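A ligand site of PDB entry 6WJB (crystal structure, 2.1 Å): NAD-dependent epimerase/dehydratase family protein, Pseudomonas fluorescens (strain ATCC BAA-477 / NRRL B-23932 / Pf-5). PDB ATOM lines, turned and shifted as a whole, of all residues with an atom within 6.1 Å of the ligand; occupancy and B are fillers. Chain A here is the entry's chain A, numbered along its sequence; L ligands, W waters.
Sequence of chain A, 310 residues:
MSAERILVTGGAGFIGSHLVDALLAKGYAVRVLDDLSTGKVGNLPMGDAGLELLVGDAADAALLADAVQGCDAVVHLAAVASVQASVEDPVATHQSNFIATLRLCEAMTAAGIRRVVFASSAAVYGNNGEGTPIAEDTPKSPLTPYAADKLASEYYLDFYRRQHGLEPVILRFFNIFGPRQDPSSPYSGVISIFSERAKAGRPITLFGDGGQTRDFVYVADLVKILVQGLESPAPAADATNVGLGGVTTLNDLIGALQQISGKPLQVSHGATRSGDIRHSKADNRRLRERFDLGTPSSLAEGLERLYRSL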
ATOM      1  N   VAL A  83     -18.136   4.588  -4.037  1.00  0.00           N
ATOM      2  CA  VAL A  83     -19.561   4.576  -3.784  1.00  0.00           C
ATOM      3  C   VAL A  83     -20.285   3.802  -4.880  1.00  0.00           C
ATOM      4  O   VAL A  83     -21.197   3.011  -4.605  1.00  0.00           O
ATOM      5  CB  VAL A  83     -20.086   6.023  -3.666  1.00  0.00           C
ATOM      6  CG1 VAL A  83     -21.594   6.044  -3.674  1.00  0.00           C
ATOM      7  CG2 VAL A  83     -19.570   6.660  -2.398  1.00  0.00           C
ATOM      8  N   ASN A 175     -13.580  15.878   1.160  1.00  0.00           N
ATOM      9  CA  ASN A 175     -12.933  15.480  -0.092  1.00  0.00           C
ATOM     10  C   ASN A 175     -11.411  15.498   0.050  1.00  0.00           C
ATOM     11  O   ASN A 175     -10.782  16.556  -0.045  1.00  0.00           O
ATOM     12  CB  ASN A 175     -13.398  16.370  -1.235  1.00  0.00           C
ATOM     13  CG  ASN A 175     -14.879  16.159  -1.536  1.00  0.00           C
ATOM     14  OD1 ASN A 175     -15.741  16.539  -0.734  1.00  0.00           O
ATOM     15  ND2 ASN A 175     -15.179  15.552  -2.674  1.00  0.00           N
ATOM     16  N   PRO A 186     -13.499   6.554 -13.632  1.00  0.00           N
ATOM     17  CA  PRO A 186     -14.285   7.776 -13.876  1.00  0.00           C
ATOM     18  C   PRO A 186     -14.816   8.418 -12.605  1.00  0.00           C
ATOM     19  O   PRO A 186     -15.093   9.628 -12.593  1.00  0.00           O
ATOM     20  CB  PRO A 186     -15.425   7.277 -14.771  1.00  0.00           C
ATOM     21  CG  PRO A 186     -15.517   5.805 -14.490  1.00  0.00           C
ATOM     22  CD  PRO A 186     -14.106   5.360 -14.249  1.00  0.00           C
ATOM     23  N   TYR A 187     -14.989   7.644 -11.539  1.00  0.00           N
ATOM     24  CA  TYR A 187     -15.438   8.180 -10.256  1.00  0.00           C
ATOM     25  C   TYR A 187     -14.283   8.406  -9.310  1.00  0.00           C
ATOM     26  O   TYR A 187     -14.494   8.517  -8.095  1.00  0.00           O
ATOM     27  CB  TYR A 187     -16.489   7.258  -9.633  1.00  0.00           C
ATOM     28  CG  TYR A 187     -17.601   6.898 -10.581  1.00  0.00           C
ATOM     29  CD1 TYR A 187     -18.560   7.836 -10.959  1.00  0.00           C
ATOM     30  CD2 TYR A 187     -17.678   5.620 -11.125  1.00  0.00           C
ATOM     31  CE1 TYR A 187     -19.572   7.500 -11.839  1.00  0.00           C
ATOM     32  CE2 TYR A 187     -18.690   5.283 -12.005  1.00  0.00           C
ATOM     33  CZ  TYR A 187     -19.628   6.223 -12.357  1.00  0.00           C
ATOM     34  OH  TYR A 187     -20.628   5.879 -13.238  1.00  0.00           O
ATOM     35  N   SER A 188     -13.056   8.462  -9.819  1.00  0.00           N
ATOM     36  CA  SER A 188     -11.951   8.959  -9.012  1.00  0.00           C
ATOM     37  C   SER A 188     -12.243  10.394  -8.596  1.00  0.00           C
ATOM     38  O   SER A 188     -13.083  11.073  -9.203  1.00  0.00           O
ATOM     39  CB  SER A 188     -10.640   8.881  -9.790  1.00  0.00           C
ATOM     40  OG  SER A 188     -10.427   7.592 -10.336  1.00  0.00           O
ATOM     41  N   GLY A 189     -11.559  10.853  -7.564  1.00  0.00           N
ATOM     42  CA  GLY A 189     -11.754  12.226  -7.121  1.00  0.00           C
ATOM     43  C   GLY A 189     -11.436  13.194  -8.250  1.00  0.00           C
ATOM     44  O   GLY A 189     -10.534  12.954  -9.059  1.00  0.00           O
ATOM     45  N   VAL A 190     -12.205  14.289  -8.327  1.00  0.00           N
ATOM     46  CA  VAL A 190     -12.073  15.208  -9.464  1.00  0.00           C
ATOM     47  C   VAL A 190     -10.683  15.816  -9.537  1.00  0.00           C
ATOM     48  O   VAL A 190     -10.185  16.123 -10.621  1.00  0.00           O
ATOM     49  CB  VAL A 190     -13.166  16.291  -9.425  1.00  0.00           C
ATOM     50  CG1 VAL A 190     -12.965  17.224  -8.230  1.00  0.00           C
ATOM     51  CG2 VAL A 190     -13.195  17.076 -10.735  1.00  0.00           C
ATOM     52  N   ILE A 191     -10.014  15.977  -8.392  1.00  0.00           N
ATOM     53  CA  ILE A 191      -8.684  16.570  -8.410  1.00  0.00           C
ATOM     54  C   ILE A 191      -7.668  15.610  -9.020  1.00  0.00           C
ATOM     55  O   ILE A 191      -6.812  16.016  -9.807  1.00  0.00           O
ATOM     56  CB  ILE A 191      -8.272  17.036  -7.001  1.00  0.00           C
ATOM     57  CG1 ILE A 191      -9.059  18.300  -6.625  1.00  0.00           C
ATOM     58  CG2 ILE A 191      -6.784  17.332  -6.943  1.00  0.00           C
ATOM     59  CD1 ILE A 191      -8.702  18.901  -5.259  1.00  0.00           C
ATOM     60  N   ILE A 193      -8.273  13.285 -11.231  1.00  0.00           N
ATOM     61  CA  ILE A 193      -8.544  13.219 -12.665  1.00  0.00           C
ATOM     62  C   ILE A 193      -8.087  14.490 -13.361  1.00  0.00           C
ATOM     63  O   ILE A 193      -7.357  14.445 -14.362  1.00  0.00           O
ATOM     64  CB  ILE A 193     -10.039  12.960 -12.916  1.00  0.00           C
ATOM     65  CG1 ILE A 193     -10.447  11.601 -12.346  1.00  0.00           C
ATOM     66  CG2 ILE A 193     -10.371  13.057 -14.401  1.00  0.00           C
ATOM     67  CD1 ILE A 193     -11.944  11.408 -12.245  1.00  0.00           C
ATOM     68  N   PHE A 194      -8.521  15.662 -12.868  1.00  0.00           N
ATOM     69  CA  PHE A 194      -8.154  16.912 -13.517  1.00  0.00           C
ATOM     70  C   PHE A 194      -6.638  17.122 -13.541  1.00  0.00           C
ATOM     71  O   PHE A 194      -6.103  17.672 -14.510  1.00  0.00           O
ATOM     72  CB  PHE A 194      -8.852  18.098 -12.844  1.00  0.00           C
ATOM     73  CG  PHE A 194     -10.298  18.281 -13.227  1.00  0.00           C
ATOM     74  CD1 PHE A 194     -10.949  17.359 -14.020  1.00  0.00           C
ATOM     75  CD2 PHE A 194     -11.012  19.384 -12.777  1.00  0.00           C
ATOM     76  CE1 PHE A 194     -12.287  17.530 -14.373  1.00  0.00           C
ATOM     77  CE2 PHE A 194     -12.340  19.569 -13.127  1.00  0.00           C
ATOM     78  CZ  PHE A 194     -12.980  18.639 -13.922  1.00  0.00           C
ATOM     79  N   THR A 205     -13.261  16.854 -18.612  1.00  0.00           N
ATOM     80  CA  THR A 205     -14.705  16.994 -18.794  1.00  0.00           C
ATOM     81  C   THR A 205     -15.292  17.584 -17.524  1.00  0.00           C
ATOM     82  O   THR A 205     -15.119  17.019 -16.433  1.00  0.00           O
ATOM     83  CB  THR A 205     -15.359  15.659 -19.137  1.00  0.00           C
ATOM     84  OG1 THR A 205     -14.714  15.077 -20.276  1.00  0.00           O
ATOM     85  CG2 THR A 205     -16.835  15.890 -19.456  1.00  0.00           C
ATOM     86  N   LEU A 206     -15.985  18.706 -17.665  1.00  0.00           N
ATOM     87  CA  LEU A 206     -16.656  19.378 -16.563  1.00  0.00           C
ATOM     88  C   LEU A 206     -18.142  19.038 -16.627  1.00  0.00           C
ATOM     89  O   LEU A 206     -18.813  19.352 -17.616  1.00  0.00           O
ATOM     90  CB  LEU A 206     -16.437  20.882 -16.646  1.00  0.00           C
ATOM     91  CG  LEU A 206     -17.001  21.748 -15.529  1.00  0.00           C
ATOM     92  CD1 LEU A 206     -16.306  21.432 -14.201  1.00  0.00           C
ATOM     93  CD2 LEU A 206     -16.862  23.219 -15.884  1.00  0.00           C
ATOM     94  N   PHE A 207     -18.639  18.375 -15.579  1.00  0.00           N
ATOM     95  CA  PHE A 207     -20.050  18.024 -15.478  1.00  0.00           C
ATOM     96  C   PHE A 207     -20.785  19.170 -14.799  1.00  0.00           C
ATOM     97  O   PHE A 207     -20.684  19.362 -13.583  1.00  0.00           O
ATOM     98  CB  PHE A 207     -20.221  16.717 -14.708  1.00  0.00           C
ATOM     99  CG  PHE A 207     -19.588  15.537 -15.382  1.00  0.00           C
ATOM    100  CD1 PHE A 207     -20.026  15.113 -16.621  1.00  0.00           C
ATOM    101  CD2 PHE A 207     -18.544  14.861 -14.781  1.00  0.00           C
ATOM    102  CE1 PHE A 207     -19.435  14.029 -17.253  1.00  0.00           C
ATOM    103  CE2 PHE A 207     -17.941  13.769 -15.415  1.00  0.00           C
ATOM    104  CZ  PHE A 207     -18.397  13.355 -16.640  1.00  0.00           C
ATOM    105  N   GLY A 208     -21.527  19.943 -15.583  1.00  0.00           N
ATOM    106  CA  GLY A 208     -22.181  21.123 -15.070  1.00  0.00           C
ATOM    107  C   GLY A 208     -21.410  22.387 -15.383  1.00  0.00           C
ATOM    108  O   GLY A 208     -20.506  22.421 -16.235  1.00  0.00           O
ATOM    109  N   GLN A 212     -20.070  24.235  -8.775  1.00  0.00           N
ATOM    110  CA  GLN A 212     -20.062  23.338  -7.606  1.00  0.00           C
ATOM    111  C   GLN A 212     -18.848  23.592  -6.732  1.00  0.00           C
ATOM    112  O   GLN A 212     -17.738  23.810  -7.225  1.00  0.00           O
ATOM    113  CB  GLN A 212     -20.036  21.865  -8.047  1.00  0.00           C
ATOM    114  CG  GLN A 212     -21.084  21.465  -9.036  1.00  0.00           C
ATOM    115  CD  GLN A 212     -20.534  21.396 -10.446  1.00  0.00           C
ATOM    116  OE1 GLN A 212     -20.276  22.421 -11.081  1.00  0.00           O
ATOM    117  NE2 GLN A 212     -20.362  20.167 -10.951  1.00  0.00           N
ATOM    118  N   ARG A 214     -16.520  22.263  -3.189  1.00  0.00           N
ATOM    119  CA  ARG A 214     -16.163  21.188  -2.287  1.00  0.00           C
ATOM    120  C   ARG A 214     -15.154  21.698  -1.258  1.00  0.00           C
ATOM    121  O   ARG A 214     -14.439  22.671  -1.487  1.00  0.00           O
ATOM    122  CB  ARG A 214     -15.581  19.969  -3.018  1.00  0.00           C
ATOM    123  CG  ARG A 214     -16.549  19.240  -3.954  1.00  0.00           C
ATOM    124  CD  ARG A 214     -17.680  18.541  -3.181  1.00  0.00           C
ATOM    125  NE  ARG A 214     -18.548  17.752  -4.073  1.00  0.00           N
ATOM    126  CZ  ARG A 214     -19.612  18.246  -4.705  1.00  0.00           C
ATOM    127  NH1 ARG A 214     -19.959  19.526  -4.548  1.00  0.00           N
ATOM    128  NH2 ARG A 214     -20.331  17.460  -5.493  1.00  0.00           N
ATOM    129  N   PHE A 216     -12.072  20.646   0.032  1.00  0.00           N
ATOM    130  CA  PHE A 216     -10.935  19.781  -0.251  1.00  0.00           C
ATOM    131  C   PHE A 216      -9.916  19.824   0.879  1.00  0.00           C
ATOM    132  O   PHE A 216      -9.609  20.889   1.423  1.00  0.00           O
ATOM    133  CB  PHE A 216     -10.238  20.181  -1.559  1.00  0.00           C
ATOM    134  CG  PHE A 216     -11.089  19.995  -2.788  1.00  0.00           C
ATOM    135  CD1 PHE A 216     -11.488  18.725  -3.171  1.00  0.00           C
ATOM    136  CD2 PHE A 216     -11.435  21.085  -3.575  1.00  0.00           C
ATOM    137  CE1 PHE A 216     -12.250  18.544  -4.309  1.00  0.00           C
ATOM    138  CE2 PHE A 216     -12.202  20.910  -4.725  1.00  0.00           C
ATOM    139  CZ  PHE A 216     -12.611  19.637  -5.089  1.00  0.00           C
ATOM    140  N   LEU A 250     -15.245  24.261  -8.886  1.00  0.00           N
ATOM    141  CA  LEU A 250     -14.539  23.484  -9.903  1.00  0.00           C
ATOM    142  C   LEU A 250     -13.855  24.412 -10.895  1.00  0.00           C
ATOM    143  O   LEU A 250     -12.755  24.119 -11.360  1.00  0.00           O
ATOM    144  CB  LEU A 250     -15.496  22.543 -10.618  1.00  0.00           C
ATOM    145  CG  LEU A 250     -16.049  21.379  -9.789  1.00  0.00           C
ATOM    146  CD1 LEU A 250     -16.774  20.391 -10.685  1.00  0.00           C
ATOM    147  CD2 LEU A 250     -14.951  20.675  -9.005  1.00  0.00           C
ATOM    148  N   THR A 272     -24.515  17.990 -15.741  1.00  0.00           N
ATOM    149  CA  THR A 272     -24.285  17.771 -14.322  1.00  0.00           C
ATOM    150  C   THR A 272     -24.701  16.349 -13.944  1.00  0.00           C
ATOM    151  O   THR A 272     -25.684  15.820 -14.454  1.00  0.00           O
ATOM    152  CB  THR A 272     -25.055  18.793 -13.485  1.00  0.00           C
ATOM    153  OG1 THR A 272     -26.282  18.222 -13.014  1.00  0.00           O
ATOM    154  CG2 THR A 272     -25.383  20.020 -14.306  1.00  0.00           C
ATOM    155  N   ARG A 273     -23.909  15.720 -13.075  1.00  0.00           N
ATOM    156  CA  ARG A 273     -24.198  14.349 -12.661  1.00  0.00           C
ATOM    157  C   ARG A 273     -25.498  14.296 -11.885  1.00  0.00           C
ATOM    158  O   ARG A 273     -25.815  15.187 -11.092  1.00  0.00           O
ATOM    159  CB  ARG A 273     -23.042  13.801 -11.807  1.00  0.00           C
ATOM    160  CG  ARG A 273     -21.867  13.276 -12.638  1.00  0.00           C
ATOM    161  CD  ARG A 273     -20.717  12.731 -11.772  1.00  0.00           C
ATOM    162  NE  ARG A 273     -19.741  12.002 -12.589  1.00  0.00           N
ATOM    163  CZ  ARG A 273     -18.519  11.655 -12.187  1.00  0.00           C
ATOM    164  NH1 ARG A 273     -18.097  11.949 -10.963  1.00  0.00           N
ATOM    165  NH2 ARG A 273     -17.716  10.990 -13.012  1.00  0.00           N
ATOM    166  N   ASP A 276     -25.856  14.936  -7.997  1.00  0.00           N
ATOM    167  CA  ASP A 276     -24.664  15.664  -7.566  1.00  0.00           C
ATOM    168  C   ASP A 276     -25.020  16.785  -6.596  1.00  0.00           C
ATOM    169  O   ASP A 276     -25.990  17.520  -6.797  1.00  0.00           O
ATOM    170  CB  ASP A 276     -23.970  16.223  -8.818  1.00  0.00           C
ATOM    171  CG  ASP A 276     -22.674  16.938  -8.511  1.00  0.00           C
ATOM    172  OD1 ASP A 276     -21.905  16.470  -7.636  1.00  0.00           O
ATOM    173  OD2 ASP A 276     -22.395  17.962  -9.191  1.00  0.00           O
ATOM    174  N   ILE A 277     -24.271  16.881  -5.503  1.00  0.00           N
ATOM    175  CA  ILE A 277     -24.441  17.969  -4.548  1.00  0.00           C
ATOM    176  C   ILE A 277     -23.714  19.196  -5.090  1.00  0.00           C
ATOM    177  O   ILE A 277     -22.556  19.099  -5.508  1.00  0.00           O
ATOM    178  CB  ILE A 277     -23.908  17.567  -3.163  1.00  0.00           C
ATOM    179  CG1 ILE A 277     -24.615  16.311  -2.662  1.00  0.00           C
ATOM    180  CG2 ILE A 277     -24.077  18.712  -2.163  1.00  0.00           C
ATOM    181  CD1 ILE A 277     -24.229  15.933  -1.249  1.00  0.00           C
ATOM    182  N   SER A 280     -20.905  21.776  -0.978  1.00  0.00           N
ATOM    183  CA  SER A 280     -20.571  20.901   0.138  1.00  0.00           C
ATOM    184  C   SER A 280     -19.434  21.525   0.952  1.00  0.00           C
ATOM    185  O   SER A 280     -18.340  21.725   0.423  1.00  0.00           O
ATOM    186  CB  SER A 280     -20.158  19.517  -0.341  1.00  0.00           C
ATOM    187  OG  SER A 280     -19.523  18.789   0.685  1.00  0.00           O
HETATM  188  C1  LIG L   1     -17.295  11.977  -3.395  1.00  0.00           C
HETATM  189  O1  LIG L   1     -18.137  12.602  -4.319  1.00  0.00           O
HETATM  190  N1  LIG L   1     -16.494  16.066 -11.780  1.00  0.00           N
HETATM  191  C2  LIG L   1     -16.293  16.652 -13.092  1.00  0.00           C
HETATM  192  N2  LIG L   1     -15.451  15.972 -13.951  1.00  0.00           N
HETATM  193  C3  LIG L   1     -14.847  14.838 -13.603  1.00  0.00           C
HETATM  194  C4  LIG L   1     -15.053  14.253 -12.238  1.00  0.00           C
HETATM  195  C5  LIG L   1     -15.889  14.927 -11.367  1.00  0.00           C
HETATM  196  O2  LIG L   1     -16.826  17.682 -13.473  1.00  0.00           O
HETATM  197  O3  LIG L   1     -14.112  14.283 -14.402  1.00  0.00           O
HETATM  198  C6  LIG L   1     -17.337  16.746 -10.826  1.00  0.00           C
HETATM  199  C7  LIG L   1     -18.433  15.958 -10.243  1.00  0.00           C
HETATM  200  O4  LIG L   1     -19.555  15.948 -11.069  1.00  0.00           O
HETATM  201  C8  LIG L   1     -18.696  16.692  -8.971  1.00  0.00           C
HETATM  202  C9  LIG L   1     -17.364  17.208  -8.584  1.00  0.00           C
HETATM  203  O5  LIG L   1     -16.567  17.198  -9.742  1.00  0.00           O
HETATM  204  O6  LIG L   1     -19.539  17.783  -9.170  1.00  0.00           O
HETATM  205  C10 LIG L   1     -16.728  16.431  -7.445  1.00  0.00           C
HETATM  206  O7  LIG L   1     -16.672  15.075  -7.806  1.00  0.00           O
HETATM  207  P1  LIG L   1     -16.024  13.985  -6.841  1.00  0.00           P
HETATM  208  O8  LIG L   1     -14.526  14.166  -6.828  1.00  0.00           O
HETATM  209  O9  LIG L   1     -16.427  12.638  -7.355  1.00  0.00           O
HETATM  210  O10 LIG L   1     -16.493  14.145  -5.345  1.00  0.00           O
HETATM  211  P2  LIG L   1     -17.924  14.129  -4.688  1.00  0.00           P
HETATM  212  O11 LIG L   1     -18.900  14.629  -5.708  1.00  0.00           O
HETATM  213  O12 LIG L   1     -17.980  15.045  -3.470  1.00  0.00           O
HETATM  214  O   HOH W   1     -18.959  12.637  -8.506  1.00  0.00           O
HETATM  215  O   HOH W   2     -13.088  14.542  -4.308  1.00  0.00           O
HETATM  216  O   HOH W   3     -21.048  13.978  -7.690  1.00  0.00           O
HETATM  217  O   HOH W   4     -12.665  15.082 -16.897  1.00  0.00           O
HETATM  218  O   HOH W   5     -21.957  17.500 -11.776  1.00  0.00           O
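CA of Gly 189 touches O8 of the ligand, at 3.4 Å. CG2 of Ile 193 touches O3 of the ligand, at 3.9 Å. Phe 194 touches the ligand (CE1 to N2, 3.6 Å). Leu 206 touches the ligand. Leu 250 touches the ligand. Arg 273 touches the ligand (CD to O4, 3.5 Å). Hydrophobic or aromatic side chains within 4 Å of the ligand: Val 190, Ile 193, Phe 194, Leu 206, Phe 207 and Leu 250. The nearest printed residue that does not touch the ligand is Ser 188 (4.1 Å).
O of Thr 205 is in hydrogen-bond range of N2 of the ligand. The backbone NH (N) of Val 190 lies within hydrogen-bond range of an oxygen (O8) of the ligand, at 2.8 Å. The guanidinium group (NE) of Arg 214 is in salt-bridge range of an oxygen (O12) of the ligand, at 2.8 Å. O6 of the ligand is in hydrogen-bond range of OD2 of Asp 276. The backbone NH (N) of Phe 207 lies within hydrogen-bond range of an oxygen (O2) of the ligand (2.9 Å). ND2 of Asn 175 lies within hydrogen-bond range of O12 of the ligand, at 3.0 Å. O6 of the ligand is in hydrogen-bond range of NE2 of Gln 212, 3.1 Å away.
Water W1 lies within hydrogen-bond range of the guanidinium group (NH1) of Arg 273 (2.7 Å) and an oxygen (O9) of the ligand (2.8 Å). Water W2 lies within hydrogen-bond range of ND2 of Asn 175 (2.8 Å) and O8 of the ligand (2.9 Å). Water W5 lies within hydrogen-bond range of the side-chain carboxylate (OD2) of Asp 276 (2.7 Å), the backbone carbonyl oxygen (O) of Phe 207 (2.9 Å), the backbone NH (N) of Arg 273 (2.9 Å), an oxygen (O4) of the ligand (2.9 Å) and the side-chain amide nitrogen (NE2) of Gln 212 (3.2 Å). Water W4 bridges the backbone NH of Thr 205 (2.5 Å) and an oxygen (O3) of the ligand (3.0 Å). Water W3 bridges the side-chain carboxylate (OD1) of Asp 276 (2.6 Å) and an oxygen (O11) of the ligand (3.0 Å).
OD1 of Asp 276 is in salt-bridge range of NH2 of Arg 214 (2.8 Å). The guanidinium group (NH2) of Arg 214 lies within hydrogen-bond range of the backbone carbonyl oxygen (O) of Ile 277 (2.8 Å). The side-chain carboxylate of Asp 276 is in hydrogen-bond range of the side-chain amide nitrogen of Gln 212 (3.5 Å). The side-chain amide nitrogen of Gln 212 is in hydrogen-bond range of the backbone carbonyl oxygen of Phe 207 (2.8 Å). The backbone carbonyl oxygen (O) of Gln 212 sits at hydrogen-bond distance from the backbone NH (N) of Leu 250, at 3.0 Å. The backbone carbonyl oxygen (O) of Pro 186 is in hydrogen-bond range of the guanidinium group (NH2) of Arg 273 (3.0 Å).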
